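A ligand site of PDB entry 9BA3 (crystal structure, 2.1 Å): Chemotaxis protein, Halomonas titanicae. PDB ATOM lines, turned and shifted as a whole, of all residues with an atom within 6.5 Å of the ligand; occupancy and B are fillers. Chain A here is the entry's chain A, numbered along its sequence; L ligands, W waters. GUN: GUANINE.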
ATOM      1  N   LEU A  83       1.278   5.659  32.110  1.00  0.00           N
ATOM      2  CA  LEU A  83       2.614   5.635  31.554  1.00  0.00           C
ATOM      3  C   LEU A  83       3.432   6.796  32.080  1.00  0.00           C
ATOM      4  O   LEU A  83       2.893   7.833  32.482  1.00  0.00           O
ATOM      5  CB  LEU A  83       2.582   5.653  30.012  1.00  0.00           C
ATOM      6  CG  LEU A  83       2.034   6.873  29.280  1.00  0.00           C
ATOM      7  CD1 LEU A  83       3.125   7.900  28.997  1.00  0.00           C
ATOM      8  CD2 LEU A  83       1.353   6.467  27.978  1.00  0.00           C
ATOM      9  N   PHE A  85       7.127   8.858  30.756  1.00  0.00           N
ATOM     10  CA  PHE A  85       7.983   8.989  29.582  1.00  0.00           C
ATOM     11  C   PHE A  85       9.191   9.856  29.902  1.00  0.00           C
ATOM     12  O   PHE A  85       9.161  10.701  30.811  1.00  0.00           O
ATOM     13  CB  PHE A  85       7.200   9.572  28.383  1.00  0.00           C
ATOM     14  CG  PHE A  85       6.813  11.012  28.567  1.00  0.00           C
ATOM     15  CD1 PHE A  85       7.665  12.039  28.163  1.00  0.00           C
ATOM     16  CD2 PHE A  85       5.601  11.352  29.142  1.00  0.00           C
ATOM     17  CE1 PHE A  85       7.314  13.364  28.336  1.00  0.00           C
ATOM     18  CE2 PHE A  85       5.241  12.675  29.316  1.00  0.00           C
ATOM     19  CZ  PHE A  85       6.108  13.683  28.917  1.00  0.00           C
ATOM     20  N   ALA A  87      12.055  12.035  27.431  1.00  0.00           N
ATOM     21  CA  ALA A  87      12.558  12.464  26.122  1.00  0.00           C
ATOM     22  C   ALA A  87      13.883  13.195  26.357  1.00  0.00           C
ATOM     23  O   ALA A  87      13.888  14.348  26.785  1.00  0.00           O
ATOM     24  CB  ALA A  87      11.563  13.354  25.402  1.00  0.00           C
ATOM     25  N   TYR A  96      13.394   8.830  23.081  1.00  0.00           N
ATOM     26  CA  TYR A  96      12.124   8.729  23.784  1.00  0.00           C
ATOM     27  C   TYR A  96      12.027   7.377  24.460  1.00  0.00           C
ATOM     28  O   TYR A  96      12.188   6.342  23.803  1.00  0.00           O
ATOM     29  CB  TYR A  96      10.965   8.950  22.817  1.00  0.00           C
ATOM     30  CG  TYR A  96       9.593   8.993  23.462  1.00  0.00           C
ATOM     31  CD1 TYR A  96       9.146  10.134  24.101  1.00  0.00           C
ATOM     32  CD2 TYR A  96       8.746   7.889  23.417  1.00  0.00           C
ATOM     33  CE1 TYR A  96       7.891  10.181  24.691  1.00  0.00           C
ATOM     34  CE2 TYR A  96       7.494   7.926  24.005  1.00  0.00           C
ATOM     35  CZ  TYR A  96       7.075   9.076  24.631  1.00  0.00           C
ATOM     36  OH  TYR A  96       5.831   9.117  25.208  1.00  0.00           O
ATOM     37  N   GLN A  98       9.656   5.024  27.433  1.00  0.00           N
ATOM     38  CA  GLN A  98       8.358   4.978  28.086  1.00  0.00           C
ATOM     39  C   GLN A  98       8.278   3.698  28.903  1.00  0.00           C
ATOM     40  O   GLN A  98       8.714   2.637  28.450  1.00  0.00           O
ATOM     41  CB  GLN A  98       7.230   5.040  27.052  1.00  0.00           C
ATOM     42  CG  GLN A  98       5.859   5.228  27.636  1.00  0.00           C
ATOM     43  CD  GLN A  98       4.777   5.212  26.574  1.00  0.00           C
ATOM     44  OE1 GLN A  98       4.037   4.239  26.452  1.00  0.00           O
ATOM     45  NE2 GLN A  98       4.684   6.288  25.813  1.00  0.00           N
ATOM     46  N   ARG A 107      12.487   4.494  21.515  1.00  0.00           N
ATOM     47  CA  ARG A 107      12.578   4.831  20.094  1.00  0.00           C
ATOM     48  C   ARG A 107      13.256   6.192  19.994  1.00  0.00           C
ATOM     49  O   ARG A 107      13.458   6.884  21.003  1.00  0.00           O
ATOM     50  CB  ARG A 107      11.200   4.879  19.427  1.00  0.00           C
ATOM     51  CG  ARG A 107      10.310   5.979  19.975  1.00  0.00           C
ATOM     52  CD  ARG A 107       9.004   6.114  19.199  1.00  0.00           C
ATOM     53  NE  ARG A 107       8.268   7.273  19.664  1.00  0.00           N
ATOM     54  CZ  ARG A 107       8.414   8.492  19.166  1.00  0.00           C
ATOM     55  NH1 ARG A 107       9.194   8.730  18.119  1.00  0.00           N
ATOM     56  NH2 ARG A 107       7.783   9.510  19.741  1.00  0.00           N
ATOM     57  N   GLU A 115       4.948  12.673  13.556  1.00  0.00           N
ATOM     58  CA  GLU A 115       4.099  12.513  14.725  1.00  0.00           C
ATOM     59  C   GLU A 115       4.700  13.072  15.998  1.00  0.00           C
ATOM     60  O   GLU A 115       4.001  13.127  17.015  1.00  0.00           O
ATOM     61  CB  GLU A 115       3.813  11.031  14.949  1.00  0.00           C
ATOM     62  CG  GLU A 115       5.056  10.285  15.392  1.00  0.00           C
ATOM     63  CD  GLU A 115       4.801   8.823  15.656  1.00  0.00           C
ATOM     64  OE1 GLU A 115       3.643   8.382  15.521  1.00  0.00           O
ATOM     65  OE2 GLU A 115       5.768   8.115  16.008  1.00  0.00           O
ATOM     66  N   ASP A 116       5.979  13.461  15.987  1.00  0.00           N
ATOM     67  CA  ASP A 116       6.639  13.997  17.168  1.00  0.00           C
ATOM     68  C   ASP A 116       6.662  15.513  17.197  1.00  0.00           C
ATOM     69  O   ASP A 116       7.496  16.109  17.885  1.00  0.00           O
ATOM     70  CB  ASP A 116       8.061  13.443  17.268  1.00  0.00           C
ATOM     71  CG  ASP A 116       8.089  11.984  17.699  1.00  0.00           C
ATOM     72  OD1 ASP A 116       7.253  11.584  18.526  1.00  0.00           O
ATOM     73  OD2 ASP A 116       8.932  11.222  17.174  1.00  0.00           O
ATOM     74  N   TRP A 118       4.774  17.319  18.762  1.00  0.00           N
ATOM     75  CA  TRP A 118       4.554  17.729  20.143  1.00  0.00           C
ATOM     76  C   TRP A 118       5.850  18.152  20.806  1.00  0.00           C
ATOM     77  O   TRP A 118       5.892  19.146  21.543  1.00  0.00           O
ATOM     78  CB  TRP A 118       3.887  16.605  20.937  1.00  0.00           C
ATOM     79  CG  TRP A 118       4.785  15.404  21.167  1.00  0.00           C
ATOM     80  CD1 TRP A 118       4.899  14.296  20.383  1.00  0.00           C
ATOM     81  CD2 TRP A 118       5.702  15.211  22.262  1.00  0.00           C
ATOM     82  NE1 TRP A 118       5.821  13.422  20.922  1.00  0.00           N
ATOM     83  CE2 TRP A 118       6.320  13.968  22.075  1.00  0.00           C
ATOM     84  CE3 TRP A 118       6.042  15.977  23.385  1.00  0.00           C
ATOM     85  CZ2 TRP A 118       7.279  13.468  22.957  1.00  0.00           C
ATOM     86  CZ3 TRP A 118       6.992  15.475  24.268  1.00  0.00           C
ATOM     87  CH2 TRP A 118       7.597  14.234  24.053  1.00  0.00           C
ATOM     88  N   TYR A 119       6.943  17.436  20.520  1.00  0.00           N
ATOM     89  CA  TYR A 119       8.216  17.697  21.184  1.00  0.00           C
ATOM     90  C   TYR A 119       8.803  19.036  20.737  1.00  0.00           C
ATOM     91  O   TYR A 119       9.288  19.811  21.567  1.00  0.00           O
ATOM     92  CB  TYR A 119       9.204  16.559  20.922  1.00  0.00           C
ATOM     93  CG  TYR A 119      10.593  16.777  21.504  1.00  0.00           C
ATOM     94  CD1 TYR A 119      10.852  16.501  22.846  1.00  0.00           C
ATOM     95  CD2 TYR A 119      11.636  17.236  20.719  1.00  0.00           C
ATOM     96  CE1 TYR A 119      12.120  16.689  23.388  1.00  0.00           C
ATOM     97  CE2 TYR A 119      12.910  17.437  21.252  1.00  0.00           C
ATOM     98  CZ  TYR A 119      13.139  17.155  22.587  1.00  0.00           C
ATOM     99  OH  TYR A 119      14.386  17.348  23.133  1.00  0.00           O
ATOM    100  N   LEU A 131       0.123  20.711  29.075  1.00  0.00           N
ATOM    101  CA  LEU A 131      -0.764  19.563  28.937  1.00  0.00           C
ATOM    102  C   LEU A 131      -1.094  19.390  27.459  1.00  0.00           C
ATOM    103  O   LEU A 131      -1.632  20.303  26.824  1.00  0.00           O
ATOM    104  CB  LEU A 131      -2.043  19.755  29.734  1.00  0.00           C
ATOM    105  CG  LEU A 131      -1.845  19.969  31.225  1.00  0.00           C
ATOM    106  CD1 LEU A 131      -3.199  20.040  31.913  1.00  0.00           C
ATOM    107  CD2 LEU A 131      -0.996  18.839  31.768  1.00  0.00           C
ATOM    108  N   ASN A 132      -0.767  18.226  26.914  1.00  0.00           N
ATOM    109  CA  ASN A 132      -0.942  17.985  25.487  1.00  0.00           C
ATOM    110  C   ASN A 132      -1.777  16.724  25.285  1.00  0.00           C
ATOM    111  O   ASN A 132      -1.338  15.623  25.611  1.00  0.00           O
ATOM    112  CB  ASN A 132       0.402  17.855  24.772  1.00  0.00           C
ATOM    113  CG  ASN A 132       0.263  17.914  23.281  1.00  0.00           C
ATOM    114  OD1 ASN A 132      -0.482  18.743  22.753  1.00  0.00           O
ATOM    115  ND2 ASN A 132       0.943  17.022  22.575  1.00  0.00           N
ATOM    116  N   LEU A 133      -2.977  16.904  24.746  1.00  0.00           N
ATOM    117  CA  LEU A 133      -3.804  15.783  24.339  1.00  0.00           C
ATOM    118  C   LEU A 133      -3.327  15.302  22.975  1.00  0.00           C
ATOM    119  O   LEU A 133      -3.402  16.036  21.989  1.00  0.00           O
ATOM    120  CB  LEU A 133      -5.271  16.203  24.296  1.00  0.00           C
ATOM    121  CG  LEU A 133      -6.361  15.139  24.492  1.00  0.00           C
ATOM    122  CD1 LEU A 133      -7.702  15.809  24.662  1.00  0.00           C
ATOM    123  CD2 LEU A 133      -6.407  14.198  23.315  1.00  0.00           C
ATOM    124  N   ASP A 134      -2.831  14.062  22.917  1.00  0.00           N
ATOM    125  CA  ASP A 134      -2.196  13.589  21.706  1.00  0.00           C
ATOM    126  C   ASP A 134      -2.307  12.072  21.628  1.00  0.00           C
ATOM    127  O   ASP A 134      -2.480  11.393  22.644  1.00  0.00           O
ATOM    128  CB  ASP A 134      -0.724  14.026  21.666  1.00  0.00           C
ATOM    129  CG  ASP A 134      -0.115  13.931  20.279  1.00  0.00           C
ATOM    130  OD1 ASP A 134      -0.845  13.612  19.321  1.00  0.00           O
ATOM    131  OD2 ASP A 134       1.104  14.181  20.154  1.00  0.00           O
ATOM    132  N   SER A 135      -2.228  11.540  20.411  1.00  0.00           N
ATOM    133  CA  SER A 135      -2.161  10.101  20.228  1.00  0.00           C
ATOM    134  C   SER A 135      -0.761   9.599  20.543  1.00  0.00           C
ATOM    135  O   SER A 135       0.239  10.309  20.359  1.00  0.00           O
ATOM    136  CB  SER A 135      -2.551   9.720  18.799  1.00  0.00           C
ATOM    137  OG  SER A 135      -1.754  10.411  17.855  1.00  0.00           O
ATOM    138  N   ASP A 136      -0.688   8.375  21.052  1.00  0.00           N
ATOM    139  CA  ASP A 136       0.581   7.815  21.477  1.00  0.00           C
ATOM    140  C   ASP A 136       1.438   7.411  20.278  1.00  0.00           C
ATOM    141  O   ASP A 136       0.916   7.084  19.210  1.00  0.00           O
ATOM    142  CB  ASP A 136       0.362   6.594  22.381  1.00  0.00           C
ATOM    143  CG  ASP A 136       1.621   6.142  23.068  1.00  0.00           C
ATOM    144  OD1 ASP A 136       2.067   6.861  23.998  1.00  0.00           O
ATOM    145  OD2 ASP A 136       2.169   5.080  22.702  1.00  0.00           O
ATOM    146  N   THR A 137       2.747   7.452  20.458  1.00  0.00           N
ATOM    147  CA  THR A 137       3.678   7.136  19.384  1.00  0.00           C
ATOM    148  C   THR A 137       4.073   5.667  19.316  1.00  0.00           C
ATOM    149  O   THR A 137       4.492   5.204  18.258  1.00  0.00           O
ATOM    150  CB  THR A 137       4.926   8.014  19.507  1.00  0.00           C
ATOM    151  OG1 THR A 137       5.495   7.854  20.815  1.00  0.00           O
ATOM    152  CG2 THR A 137       4.568   9.469  19.282  1.00  0.00           C
ATOM    153  N   PHE A 144      -3.673  10.064  25.158  1.00  0.00           N
ATOM    154  CA  PHE A 144      -3.516  10.453  26.548  1.00  0.00           C
ATOM    155  C   PHE A 144      -3.416  11.969  26.618  1.00  0.00           C
ATOM    156  O   PHE A 144      -3.169  12.651  25.623  1.00  0.00           O
ATOM    157  CB  PHE A 144      -2.271   9.820  27.180  1.00  0.00           C
ATOM    158  CG  PHE A 144      -2.277   8.318  27.151  1.00  0.00           C
ATOM    159  CD1 PHE A 144      -2.894   7.594  28.158  1.00  0.00           C
ATOM    160  CD2 PHE A 144      -1.690   7.631  26.100  1.00  0.00           C
ATOM    161  CE1 PHE A 144      -2.919   6.212  28.127  1.00  0.00           C
ATOM    162  CE2 PHE A 144      -1.704   6.244  26.057  1.00  0.00           C
ATOM    163  CZ  PHE A 144      -2.324   5.537  27.077  1.00  0.00           C
ATOM    164  N   TYR A 146      -0.849  14.188  28.072  1.00  0.00           N
ATOM    165  CA  TYR A 146       0.520  14.091  28.530  1.00  0.00           C
ATOM    166  C   TYR A 146       0.911  15.330  29.317  1.00  0.00           C
ATOM    167  O   TYR A 146       0.631  16.462  28.893  1.00  0.00           O
ATOM    168  CB  TYR A 146       1.498  13.926  27.359  1.00  0.00           C
ATOM    169  CG  TYR A 146       1.310  12.652  26.551  1.00  0.00           C
ATOM    170  CD1 TYR A 146       0.419  12.616  25.491  1.00  0.00           C
ATOM    171  CD2 TYR A 146       2.034  11.506  26.842  1.00  0.00           C
ATOM    172  CE1 TYR A 146       0.247  11.471  24.740  1.00  0.00           C
ATOM    173  CE2 TYR A 146       1.856  10.348  26.100  1.00  0.00           C
ATOM    174  CZ  TYR A 146       0.960  10.339  25.056  1.00  0.00           C
ATOM    175  OH  TYR A 146       0.775   9.203  24.297  1.00  0.00           O
ATOM    176  N   VAL A 147       1.577  15.127  30.453  1.00  0.00           N
ATOM    177  CA  VAL A 147       2.149  16.210  31.234  1.00  0.00           C
ATOM    178  C   VAL A 147       3.595  16.363  30.760  1.00  0.00           C
ATOM    179  O   VAL A 147       4.484  15.624  31.190  1.00  0.00           O
ATOM    180  CB  VAL A 147       2.070  15.946  32.735  1.00  0.00           C
ATOM    181  CG1 VAL A 147       2.656  17.104  33.525  1.00  0.00           C
ATOM    182  CG2 VAL A 147       0.623  15.689  33.154  1.00  0.00           C
ATOM    183  N   ASN A 148       3.836  17.319  29.856  1.00  0.00           N
ATOM    184  CA  ASN A 148       5.170  17.563  29.307  1.00  0.00           C
ATOM    185  C   ASN A 148       5.880  18.587  30.185  1.00  0.00           C
ATOM    186  O   ASN A 148       5.596  19.785  30.097  1.00  0.00           O
ATOM    187  CB  ASN A 148       5.089  18.050  27.870  1.00  0.00           C
ATOM    188  CG  ASN A 148       4.440  17.051  26.927  1.00  0.00           C
ATOM    189  OD1 ASN A 148       3.714  17.422  26.006  1.00  0.00           O
ATOM    190  ND2 ASN A 148       4.695  15.769  27.159  1.00  0.00           N
ATOM    191  N   VAL A 163      12.812  16.134  28.790  1.00  0.00           N
ATOM    192  CA  VAL A 163      11.377  16.364  28.930  1.00  0.00           C
ATOM    193  C   VAL A 163      10.776  15.071  29.457  1.00  0.00           C
ATOM    194  O   VAL A 163      11.055  13.987  28.930  1.00  0.00           O
ATOM    195  CB  VAL A 163      10.735  16.774  27.586  1.00  0.00           C
ATOM    196  CG1 VAL A 163       9.235  16.984  27.753  1.00  0.00           C
ATOM    197  CG2 VAL A 163      11.416  18.025  27.043  1.00  0.00           C
ATOM    198  N   ALA A 166       3.981  12.252  32.824  1.00  0.00           N
ATOM    199  CA  ALA A 166       3.052  11.130  32.838  1.00  0.00           C
ATOM    200  C   ALA A 166       2.020  11.278  31.732  1.00  0.00           C
ATOM    201  O   ALA A 166       1.751  12.374  31.230  1.00  0.00           O
ATOM    202  CB  ALA A 166       2.330  11.029  34.192  1.00  0.00           C
HETATM  203  N9  GUN L   1       4.970  11.672  25.063  1.00  0.00           N
HETATM  204  C8  GUN L   1       5.198  12.683  25.941  1.00  0.00           C
HETATM  205  N7  GUN L   1       4.544  13.792  25.655  1.00  0.00           N
HETATM  206  C5  GUN L   1       3.834  13.479  24.502  1.00  0.00           C
HETATM  207  C6  GUN L   1       2.959  14.279  23.733  1.00  0.00           C
HETATM  208  O6  GUN L   1       2.627  15.450  23.923  1.00  0.00           O
HETATM  209  N1  GUN L   1       2.463  13.570  22.628  1.00  0.00           N
HETATM  210  C2  GUN L   1       2.764  12.266  22.322  1.00  0.00           C
HETATM  211  N2  GUN L   1       2.191  11.754  21.234  1.00  0.00           N
HETATM  212  N3  GUN L   1       3.591  11.524  23.054  1.00  0.00           N
HETATM  213  C4  GUN L   1       4.103  12.158  24.136  1.00  0.00           C
HETATM  214  O   HOH W   1       4.026   8.562  22.719  1.00  0.00           O
HETATM  215  O   HOH W   2       1.453  11.397  18.001  1.00  0.00           O
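The backbone carbonyl oxygen of Asn 132 is in hydrogen-bond range of the backbone NH of Tyr 146, at 2.9 Å.
The side-chain hydroxyl (OH) of Tyr 96 lies within hydrogen-bond range of the side-chain amide nitrogen (NE2) of Gln 98.
The backbone NH (N) of Tyr 96 sits at hydrogen-bond distance from the backbone carbonyl oxygen (O) of Arg 107 (2.8 Å).
O of Phe 144 lies within hydrogen-bond range of N of Asp 134, at 3.1 Å.
OD1 of Asp 116 lies within hydrogen-bond range of NE1 of Trp 118, at 3.3 Å.
OD1 of Asp 136 sits at hydrogen-bond distance from OH of Tyr 146.
OG1 of Thr 137 is in hydrogen-bond range of NH2 of Arg 107, at 3.0 Å.
Water W1 lies within hydrogen-bond range of OG1 of Thr 137, OD1 of Asp 136, N3 of the ligand and OH of Tyr 96.
Merely in contact with the ligand: Phe 85 (3.3 Å), Trp 118 (3.2 Å), Thr 137 (3.8 Å) and Tyr 146 (3.4 Å).
Hydrophobic or aromatic side chains within 4 Å of the ligand: Phe 85, Tyr 96, Trp 118 and Tyr 146.
Nine residues have an atom within 4 Å of the ligand: Phe 85, Tyr 96, Trp 118, Asn 132, Asp 134, Ser 135, Thr 137, Tyr 146 and Asn 148.
The side-chain amide nitrogen (ND2) of Asn 148 is in hydrogen-bond range of a nitrogen (N7) of the ligand (2.5 Å).
The backbone carbonyl oxygen (O) of Ser 135 lies within hydrogen-bond range of a nitrogen (N2) of the ligand, 2.6 Å away.
ND2 of Asn 132 is in hydrogen-bond range of O6 of the ligand (2.7 Å).
N9 of the ligand is in hydrogen-bond range of OH of Tyr 96, 2.7 Å away.
The side-chain carboxylate (OD2) of Asp 134 is in hydrogen-bond range of a nitrogen (N2) of the ligand, at 2.9 Å.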
